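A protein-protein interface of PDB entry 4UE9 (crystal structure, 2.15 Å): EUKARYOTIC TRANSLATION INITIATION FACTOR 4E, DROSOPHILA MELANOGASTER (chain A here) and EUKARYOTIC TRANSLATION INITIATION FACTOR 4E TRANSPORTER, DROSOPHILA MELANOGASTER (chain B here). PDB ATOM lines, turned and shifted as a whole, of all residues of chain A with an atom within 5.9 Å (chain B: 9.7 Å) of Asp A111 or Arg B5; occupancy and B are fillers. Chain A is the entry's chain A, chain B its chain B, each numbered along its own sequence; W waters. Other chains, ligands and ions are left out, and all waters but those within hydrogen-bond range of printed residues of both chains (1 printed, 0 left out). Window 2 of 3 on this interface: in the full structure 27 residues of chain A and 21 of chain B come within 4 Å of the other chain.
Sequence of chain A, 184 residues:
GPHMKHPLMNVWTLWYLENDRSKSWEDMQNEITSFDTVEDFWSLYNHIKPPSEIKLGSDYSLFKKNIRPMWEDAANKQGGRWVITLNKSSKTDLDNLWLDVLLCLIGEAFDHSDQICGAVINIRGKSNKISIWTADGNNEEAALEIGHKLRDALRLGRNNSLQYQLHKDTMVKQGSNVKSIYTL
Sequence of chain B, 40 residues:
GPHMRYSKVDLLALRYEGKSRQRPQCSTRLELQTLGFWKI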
ATOM      1  N   MET A   9     -20.265 -27.833  -1.246  1.00  0.00           N
ATOM      2  CA  MET A   9     -21.661 -27.833  -1.661  1.00  0.00           C
ATOM      3  C   MET A   9     -22.426 -28.948  -0.957  1.00  0.00           C
ATOM      4  O   MET A   9     -23.571 -28.762  -0.545  1.00  0.00           O
ATOM      5  CB  MET A   9     -21.774 -27.998  -3.178  1.00  0.00           C
ATOM      6  CG  MET A   9     -23.194 -27.845  -3.710  1.00  0.00           C
ATOM      7  SD  MET A   9     -23.374 -28.393  -5.419  1.00  0.00           S
ATOM      8  CE  MET A   9     -22.290 -27.242  -6.265  1.00  0.00           C
ATOM      9  N   GLY A 107     -15.344 -30.854  -5.221  1.00  0.00           N
ATOM     10  CA  GLY A 107     -15.279 -29.593  -5.940  1.00  0.00           C
ATOM     11  C   GLY A 107     -16.459 -29.393  -6.876  1.00  0.00           C
ATOM     12  O   GLY A 107     -16.631 -28.314  -7.443  1.00  0.00           O
ATOM     13  N   GLU A 108     -17.265 -30.440  -7.040  1.00  0.00           N
ATOM     14  CA  GLU A 108     -18.478 -30.379  -7.851  1.00  0.00           C
ATOM     15  C   GLU A 108     -18.167 -29.968  -9.290  1.00  0.00           C
ATOM     16  O   GLU A 108     -18.740 -29.015  -9.820  1.00  0.00           O
ATOM     17  CB  GLU A 108     -19.485 -29.411  -7.222  1.00  0.00           C
ATOM     18  CG  GLU A 108     -19.875 -29.786  -5.791  1.00  0.00           C
ATOM     19  CD  GLU A 108     -20.777 -31.006  -5.719  1.00  0.00           C
ATOM     20  OE1 GLU A 108     -21.260 -31.462  -6.780  1.00  0.00           O
ATOM     21  OE2 GLU A 108     -21.002 -31.511  -4.598  1.00  0.00           O
ATOM     22  N   ALA A 109     -17.259 -30.708  -9.918  1.00  0.00           N
ATOM     23  CA  ALA A 109     -16.809 -30.403 -11.272  1.00  0.00           C
ATOM     24  C   ALA A 109     -17.835 -30.805 -12.327  1.00  0.00           C
ATOM     25  O   ALA A 109     -17.649 -30.527 -13.510  1.00  0.00           O
ATOM     26  CB  ALA A 109     -15.482 -31.096 -11.545  1.00  0.00           C
ATOM     27  N   PHE A 110     -18.917 -31.453 -11.898  1.00  0.00           N
ATOM     28  CA  PHE A 110     -19.928 -31.961 -12.820  1.00  0.00           C
ATOM     29  C   PHE A 110     -21.166 -31.065 -12.858  1.00  0.00           C
ATOM     30  O   PHE A 110     -21.593 -30.538 -11.832  1.00  0.00           O
ATOM     31  CB  PHE A 110     -20.329 -33.384 -12.428  1.00  0.00           C
ATOM     32  CG  PHE A 110     -19.159 -34.287 -12.166  1.00  0.00           C
ATOM     33  CD1 PHE A 110     -18.464 -34.862 -13.216  1.00  0.00           C
ATOM     34  CD2 PHE A 110     -18.752 -34.558 -10.870  1.00  0.00           C
ATOM     35  CE1 PHE A 110     -17.384 -35.690 -12.980  1.00  0.00           C
ATOM     36  CE2 PHE A 110     -17.673 -35.387 -10.626  1.00  0.00           C
ATOM     37  CZ  PHE A 110     -16.987 -35.955 -11.684  1.00  0.00           C
ATOM     38  N   ASP A 111     -21.736 -30.901 -14.048  1.00  0.00           N
ATOM     39  CA  ASP A 111     -22.946 -30.103 -14.212  1.00  0.00           C
ATOM     40  C   ASP A 111     -24.133 -30.789 -13.550  1.00  0.00           C
ATOM     41  O   ASP A 111     -24.967 -30.137 -12.925  1.00  0.00           O
ATOM     42  CB  ASP A 111     -23.241 -29.862 -15.692  1.00  0.00           C
ATOM     43  CG  ASP A 111     -22.141 -29.086 -16.390  1.00  0.00           C
ATOM     44  OD1 ASP A 111     -21.419 -28.327 -15.710  1.00  0.00           O
ATOM     45  OD2 ASP A 111     -22.001 -29.235 -17.622  1.00  0.00           O
ATOM     46  N   HIS A 112     -24.204 -32.108 -13.700  1.00  0.00           N
ATOM     47  CA  HIS A 112     -25.244 -32.901 -13.057  1.00  0.00           C
ATOM     48  C   HIS A 112     -24.783 -33.343 -11.673  1.00  0.00           C
ATOM     49  O   HIS A 112     -24.607 -34.533 -11.419  1.00  0.00           O
ATOM     50  CB  HIS A 112     -25.598 -34.120 -13.909  1.00  0.00           C
ATOM     51  CG  HIS A 112     -26.050 -33.780 -15.297  1.00  0.00           C
ATOM     52  ND1 HIS A 112     -25.195 -33.276 -16.253  1.00  0.00           N
ATOM     53  CD2 HIS A 112     -27.262 -33.876 -15.886  1.00  0.00           C
ATOM     54  CE1 HIS A 112     -25.863 -33.075 -17.374  1.00  0.00           C
ATOM     55  NE2 HIS A 112     -27.121 -33.432 -17.180  1.00  0.00           N
ATOM     56  N   SER A 113     -24.585 -32.375 -10.782  1.00  0.00           N
ATOM     57  CA  SER A 113     -24.081 -32.653  -9.441  1.00  0.00           C
ATOM     58  C   SER A 113     -25.006 -33.588  -8.671  1.00  0.00           C
ATOM     59  O   SER A 113     -24.547 -34.450  -7.922  1.00  0.00           O
ATOM     60  CB  SER A 113     -23.899 -31.350  -8.661  1.00  0.00           C
ATOM     61  OG  SER A 113     -25.123 -30.643  -8.563  1.00  0.00           O
ATOM     62  N   ASP A 114     -26.311 -33.416  -8.861  1.00  0.00           N
ATOM     63  CA  ASP A 114     -27.299 -34.212  -8.144  1.00  0.00           C
ATOM     64  C   ASP A 114     -27.248 -35.681  -8.558  1.00  0.00           C
ATOM     65  O   ASP A 114     -27.759 -36.548  -7.851  1.00  0.00           O
ATOM     66  CB  ASP A 114     -28.705 -33.656  -8.377  1.00  0.00           C
ATOM     67  CG  ASP A 114     -28.844 -32.213  -7.933  1.00  0.00           C
ATOM     68  OD1 ASP A 114     -28.035 -31.765  -7.093  1.00  0.00           O
ATOM     69  OD2 ASP A 114     -29.764 -31.526  -8.424  1.00  0.00           O
ATOM     70  N   GLU A 145     -22.169 -36.600 -19.612  1.00  0.00           N
ATOM     71  CA  GLU A 145     -21.617 -35.324 -19.171  1.00  0.00           C
ATOM     72  C   GLU A 145     -20.606 -35.559 -18.055  1.00  0.00           C
ATOM     73  O   GLU A 145     -19.535 -34.953 -18.036  1.00  0.00           O
ATOM     74  CB  GLU A 145     -22.732 -34.385 -18.700  1.00  0.00           C
ATOM     75  CG  GLU A 145     -22.242 -33.020 -18.210  1.00  0.00           C
ATOM     76  CD  GLU A 145     -21.892 -32.996 -16.728  1.00  0.00           C
ATOM     77  OE1 GLU A 145     -22.616 -33.625 -15.926  1.00  0.00           O
ATOM     78  OE2 GLU A 145     -20.895 -32.339 -16.362  1.00  0.00           O
ATOM     79  N   LYS A 149     -16.435 -35.240 -18.268  1.00  0.00           N
ATOM     80  CA  LYS A 149     -15.725 -34.430 -17.284  1.00  0.00           C
ATOM     81  C   LYS A 149     -14.575 -35.235 -16.691  1.00  0.00           C
ATOM     82  O   LYS A 149     -13.485 -34.707 -16.465  1.00  0.00           O
ATOM     83  CB  LYS A 149     -16.667 -33.957 -16.174  1.00  0.00           C
ATOM     84  CG  LYS A 149     -17.544 -32.769 -16.551  1.00  0.00           C
ATOM     85  CD  LYS A 149     -16.716 -31.518 -16.818  1.00  0.00           C
ATOM     86  CE  LYS A 149     -17.589 -30.274 -16.870  1.00  0.00           C
ATOM     87  NZ  LYS A 149     -18.704 -30.408 -17.848  1.00  0.00           N
ATOM     88  N   PRO B   2     -26.653 -22.509  -2.598  1.00  0.00           N
ATOM     89  CA  PRO B   2     -26.154 -22.120  -3.920  1.00  0.00           C
ATOM     90  C   PRO B   2     -25.120 -23.102  -4.460  1.00  0.00           C
ATOM     91  O   PRO B   2     -24.839 -24.114  -3.816  1.00  0.00           O
ATOM     92  CB  PRO B   2     -25.530 -20.747  -3.664  1.00  0.00           C
ATOM     93  CG  PRO B   2     -25.095 -20.798  -2.246  1.00  0.00           C
ATOM     94  CD  PRO B   2     -26.105 -21.655  -1.530  1.00  0.00           C
ATOM     95  N   HIS B   3     -24.561 -22.795  -5.627  1.00  0.00           N
ATOM     96  CA  HIS B   3     -23.621 -23.689  -6.289  1.00  0.00           C
ATOM     97  C   HIS B   3     -22.175 -23.336  -5.934  1.00  0.00           C
ATOM     98  O   HIS B   3     -21.638 -22.332  -6.404  1.00  0.00           O
ATOM     99  CB  HIS B   3     -23.828 -23.636  -7.806  1.00  0.00           C
ATOM    100  CG  HIS B   3     -23.632 -24.951  -8.491  1.00  0.00           C
ATOM    101  ND1 HIS B   3     -22.532 -25.228  -9.279  1.00  0.00           N
ATOM    102  CD2 HIS B   3     -24.397 -26.069  -8.517  1.00  0.00           C
ATOM    103  CE1 HIS B   3     -22.628 -26.453  -9.755  1.00  0.00           C
ATOM    104  NE2 HIS B   3     -23.753 -26.988  -9.307  1.00  0.00           N
ATOM    105  N   MET B   4     -21.558 -24.166  -5.095  1.00  0.00           N
ATOM    106  CA  MET B   4     -20.168 -23.976  -4.687  1.00  0.00           C
ATOM    107  C   MET B   4     -19.239 -24.894  -5.472  1.00  0.00           C
ATOM    108  O   MET B   4     -19.093 -26.070  -5.139  1.00  0.00           O
ATOM    109  CB  MET B   4     -20.008 -24.241  -3.188  1.00  0.00           C
ATOM    110  CG  MET B   4     -20.698 -23.220  -2.298  1.00  0.00           C
ATOM    111  SD  MET B   4     -19.945 -21.583  -2.388  1.00  0.00           S
ATOM    112  CE  MET B   4     -18.373 -21.880  -1.583  1.00  0.00           C
ATOM    113  N   ARG B   5     -18.613 -24.349  -6.513  1.00  0.00           N
ATOM    114  CA  ARG B   5     -17.697 -25.114  -7.351  1.00  0.00           C
ATOM    115  C   ARG B   5     -16.247 -24.726  -7.075  1.00  0.00           C
ATOM    116  O   ARG B   5     -15.873 -23.559  -7.195  1.00  0.00           O
ATOM    117  CB  ARG B   5     -18.015 -24.901  -8.835  1.00  0.00           C
ATOM    118  CG  ARG B   5     -19.483 -25.075  -9.189  1.00  0.00           C
ATOM    119  CD  ARG B   5     -19.707 -24.999 -10.691  1.00  0.00           C
ATOM    120  NE  ARG B   5     -19.438 -26.272 -11.353  1.00  0.00           N
ATOM    121  CZ  ARG B   5     -19.526 -26.467 -12.666  1.00  0.00           C
ATOM    122  NH1 ARG B   5     -19.874 -25.471 -13.471  1.00  0.00           N
ATOM    123  NH2 ARG B   5     -19.266 -27.662 -13.178  1.00  0.00           N
ATOM    124  N   TYR B   6     -15.441 -25.715  -6.702  1.00  0.00           N
ATOM    125  CA  TYR B   6     -14.012 -25.516  -6.492  1.00  0.00           C
ATOM    126  C   TYR B   6     -13.212 -26.218  -7.582  1.00  0.00           C
ATOM    127  O   TYR B   6     -13.418 -27.403  -7.844  1.00  0.00           O
ATOM    128  CB  TYR B   6     -13.583 -26.046  -5.122  1.00  0.00           C
ATOM    129  CG  TYR B   6     -14.196 -25.319  -3.947  1.00  0.00           C
ATOM    130  CD1 TYR B   6     -13.579 -24.201  -3.399  1.00  0.00           C
ATOM    131  CD2 TYR B   6     -15.382 -25.758  -3.374  1.00  0.00           C
ATOM    132  CE1 TYR B   6     -14.130 -23.535  -2.321  1.00  0.00           C
ATOM    133  CE2 TYR B   6     -15.941 -25.099  -2.294  1.00  0.00           C
ATOM    134  CZ  TYR B   6     -15.311 -23.989  -1.772  1.00  0.00           C
ATOM    135  OH  TYR B   6     -15.861 -23.330  -0.698  1.00  0.00           O
ATOM    136  N   SER B   7     -12.303 -25.485  -8.215  1.00  0.00           N
ATOM    137  CA  SER B   7     -11.390 -26.082  -9.180  1.00  0.00           C
ATOM    138  C   SER B   7     -10.364 -26.925  -8.438  1.00  0.00           C
ATOM    139  O   SER B   7     -10.217 -26.800  -7.223  1.00  0.00           O
ATOM    140  CB  SER B   7     -10.691 -25.005 -10.012  1.00  0.00           C
ATOM    141  OG  SER B   7      -9.783 -24.261  -9.217  1.00  0.00           O
ATOM    142  N   LYS B   8      -9.660 -27.784  -9.167  1.00  0.00           N
ATOM    143  CA  LYS B   8      -8.600 -28.593  -8.580  1.00  0.00           C
ATOM    144  C   LYS B   8      -7.559 -27.696  -7.917  1.00  0.00           C
ATOM    145  O   LYS B   8      -7.030 -28.023  -6.855  1.00  0.00           O
ATOM    146  CB  LYS B   8      -7.944 -29.475  -9.643  1.00  0.00           C
ATOM    147  CG  LYS B   8      -6.765 -30.294  -9.139  1.00  0.00           C
ATOM    148  CD  LYS B   8      -6.158 -31.134 -10.252  1.00  0.00           C
ATOM    149  CE  LYS B   8      -4.902 -31.851  -9.784  1.00  0.00           C
ATOM    150  NZ  LYS B   8      -4.247 -32.612 -10.882  1.00  0.00           N
ATOM    151  N   VAL B   9      -7.278 -26.562  -8.552  1.00  0.00           N
ATOM    152  CA  VAL B   9      -6.300 -25.607  -8.042  1.00  0.00           C
ATOM    153  C   VAL B   9      -6.769 -25.013  -6.719  1.00  0.00           C
ATOM    154  O   VAL B   9      -6.005 -24.946  -5.759  1.00  0.00           O
ATOM    155  CB  VAL B   9      -6.041 -24.468  -9.059  1.00  0.00           C
ATOM    156  CG1 VAL B   9      -5.170 -23.370  -8.454  1.00  0.00           C
ATOM    157  CG2 VAL B   9      -5.389 -25.022 -10.313  1.00  0.00           C
ATOM    158  N   ASP B  10      -8.026 -24.580  -6.680  1.00  0.00           N
ATOM    159  CA  ASP B  10      -8.594 -23.978  -5.479  1.00  0.00           C
ATOM    160  C   ASP B  10      -8.530 -24.947  -4.306  1.00  0.00           C
ATOM    161  O   ASP B  10      -8.232 -24.552  -3.181  1.00  0.00           O
ATOM    162  CB  ASP B  10     -10.042 -23.548  -5.724  1.00  0.00           C
ATOM    163  CG  ASP B  10     -10.159 -22.436  -6.750  1.00  0.00           C
ATOM    164  OD1 ASP B  10      -9.197 -21.653  -6.898  1.00  0.00           O
ATOM    165  OD2 ASP B  10     -11.218 -22.346  -7.407  1.00  0.00           O
ATOM    166  N   LEU B  11      -8.804 -26.217  -4.580  1.00  0.00           N
ATOM    167  CA  LEU B  11      -8.817 -27.239  -3.540  1.00  0.00           C
ATOM    168  C   LEU B  11      -7.409 -27.537  -3.033  1.00  0.00           C
ATOM    169  O   LEU B  11      -7.174 -27.574  -1.824  1.00  0.00           O
ATOM    170  CB  LEU B  11      -9.473 -28.516  -4.067  1.00  0.00           C
ATOM    171  CG  LEU B  11     -10.965 -28.398  -4.393  1.00  0.00           C
ATOM    172  CD1 LEU B  11     -11.461 -29.641  -5.108  1.00  0.00           C
ATOM    173  CD2 LEU B  11     -11.782 -28.150  -3.129  1.00  0.00           C
HETATM  174  O   HOH W   1     -17.969 -27.771  -3.142  1.00  0.00           O
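The backbone NH of Tyr B6 lies within hydrogen-bond range of the backbone carbonyl oxygen of Gly A107 (3.0 Å).
O of Glu A108 is in hydrogen-bond range of NE of Arg B5, at 3.2 Å.
OD1 of Asp A111 lies within salt-bridge range of NH2 of Arg B5 (3.4 Å).
The backbone carbonyl oxygen of Ala A109 sits at hydrogen-bond distance from the guanidinium group of Arg B5 (3.3 Å).
Met A9 touches His B3 (CE to CD2, 3.3 Å).
CE of Met A9 touches N of Met B4 (3.4 Å).
Arg B5 touches Gly A107 (CA to O, 3.4 Å).
Gly A107 touches Leu B11.
O of Met B4 touches CG of Glu A108, 3.9 Å away.
Phe A110 touches Arg B5 (C to NH2, 3.9 Å).
Ser A113 touches His B3.
Water W1 bridges the backbone carbonyl oxygen of Met B4 (2.9 Å) and the backbone NH of Met A9 (3.0 Å).
OD1 of Asp A114 is in hydrogen-bond range of OG of Ser A113 (3.4 Å).
OE2 of Glu A145 is in hydrogen-bond range of N of Asp A111 (2.9 Å).
The side-chain carboxylate of Asp A111 lies within salt-bridge range of the side-chain amino group of Lys A149, 3.5 Å away.
Asp A111 touches one residue of chain B.
Arg B5 touches just these residues of chain A: Gly A107, Glu A108, Ala A109, Phe A110 and Asp A111.
Of chain B, only Arg B5 (3.3 Å) comes within 4 Å of Ala A109.
Printed residues of chain B within 4 Å of Glu A108: Met B4 and Arg B5.
Printed residues of chain B within 4 Å of Phe A110: Arg B5 (3.9 Å).
Of the printed residues of chain B, Gly A107 touches Arg B5, Tyr B6 and Leu B11.
Hydrophobic or aromatic side chains of chain B that line the printed part of chain A: His B3 and Leu B11.
Among the printed residues, 11 pairs touch across the chains.
Among the printed residues, Asp or Glu carboxylates within 4 Å of a Lys or Arg side-chain nitrogen of the other chain: Asp A111 with Arg B5 (3.4 Å).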
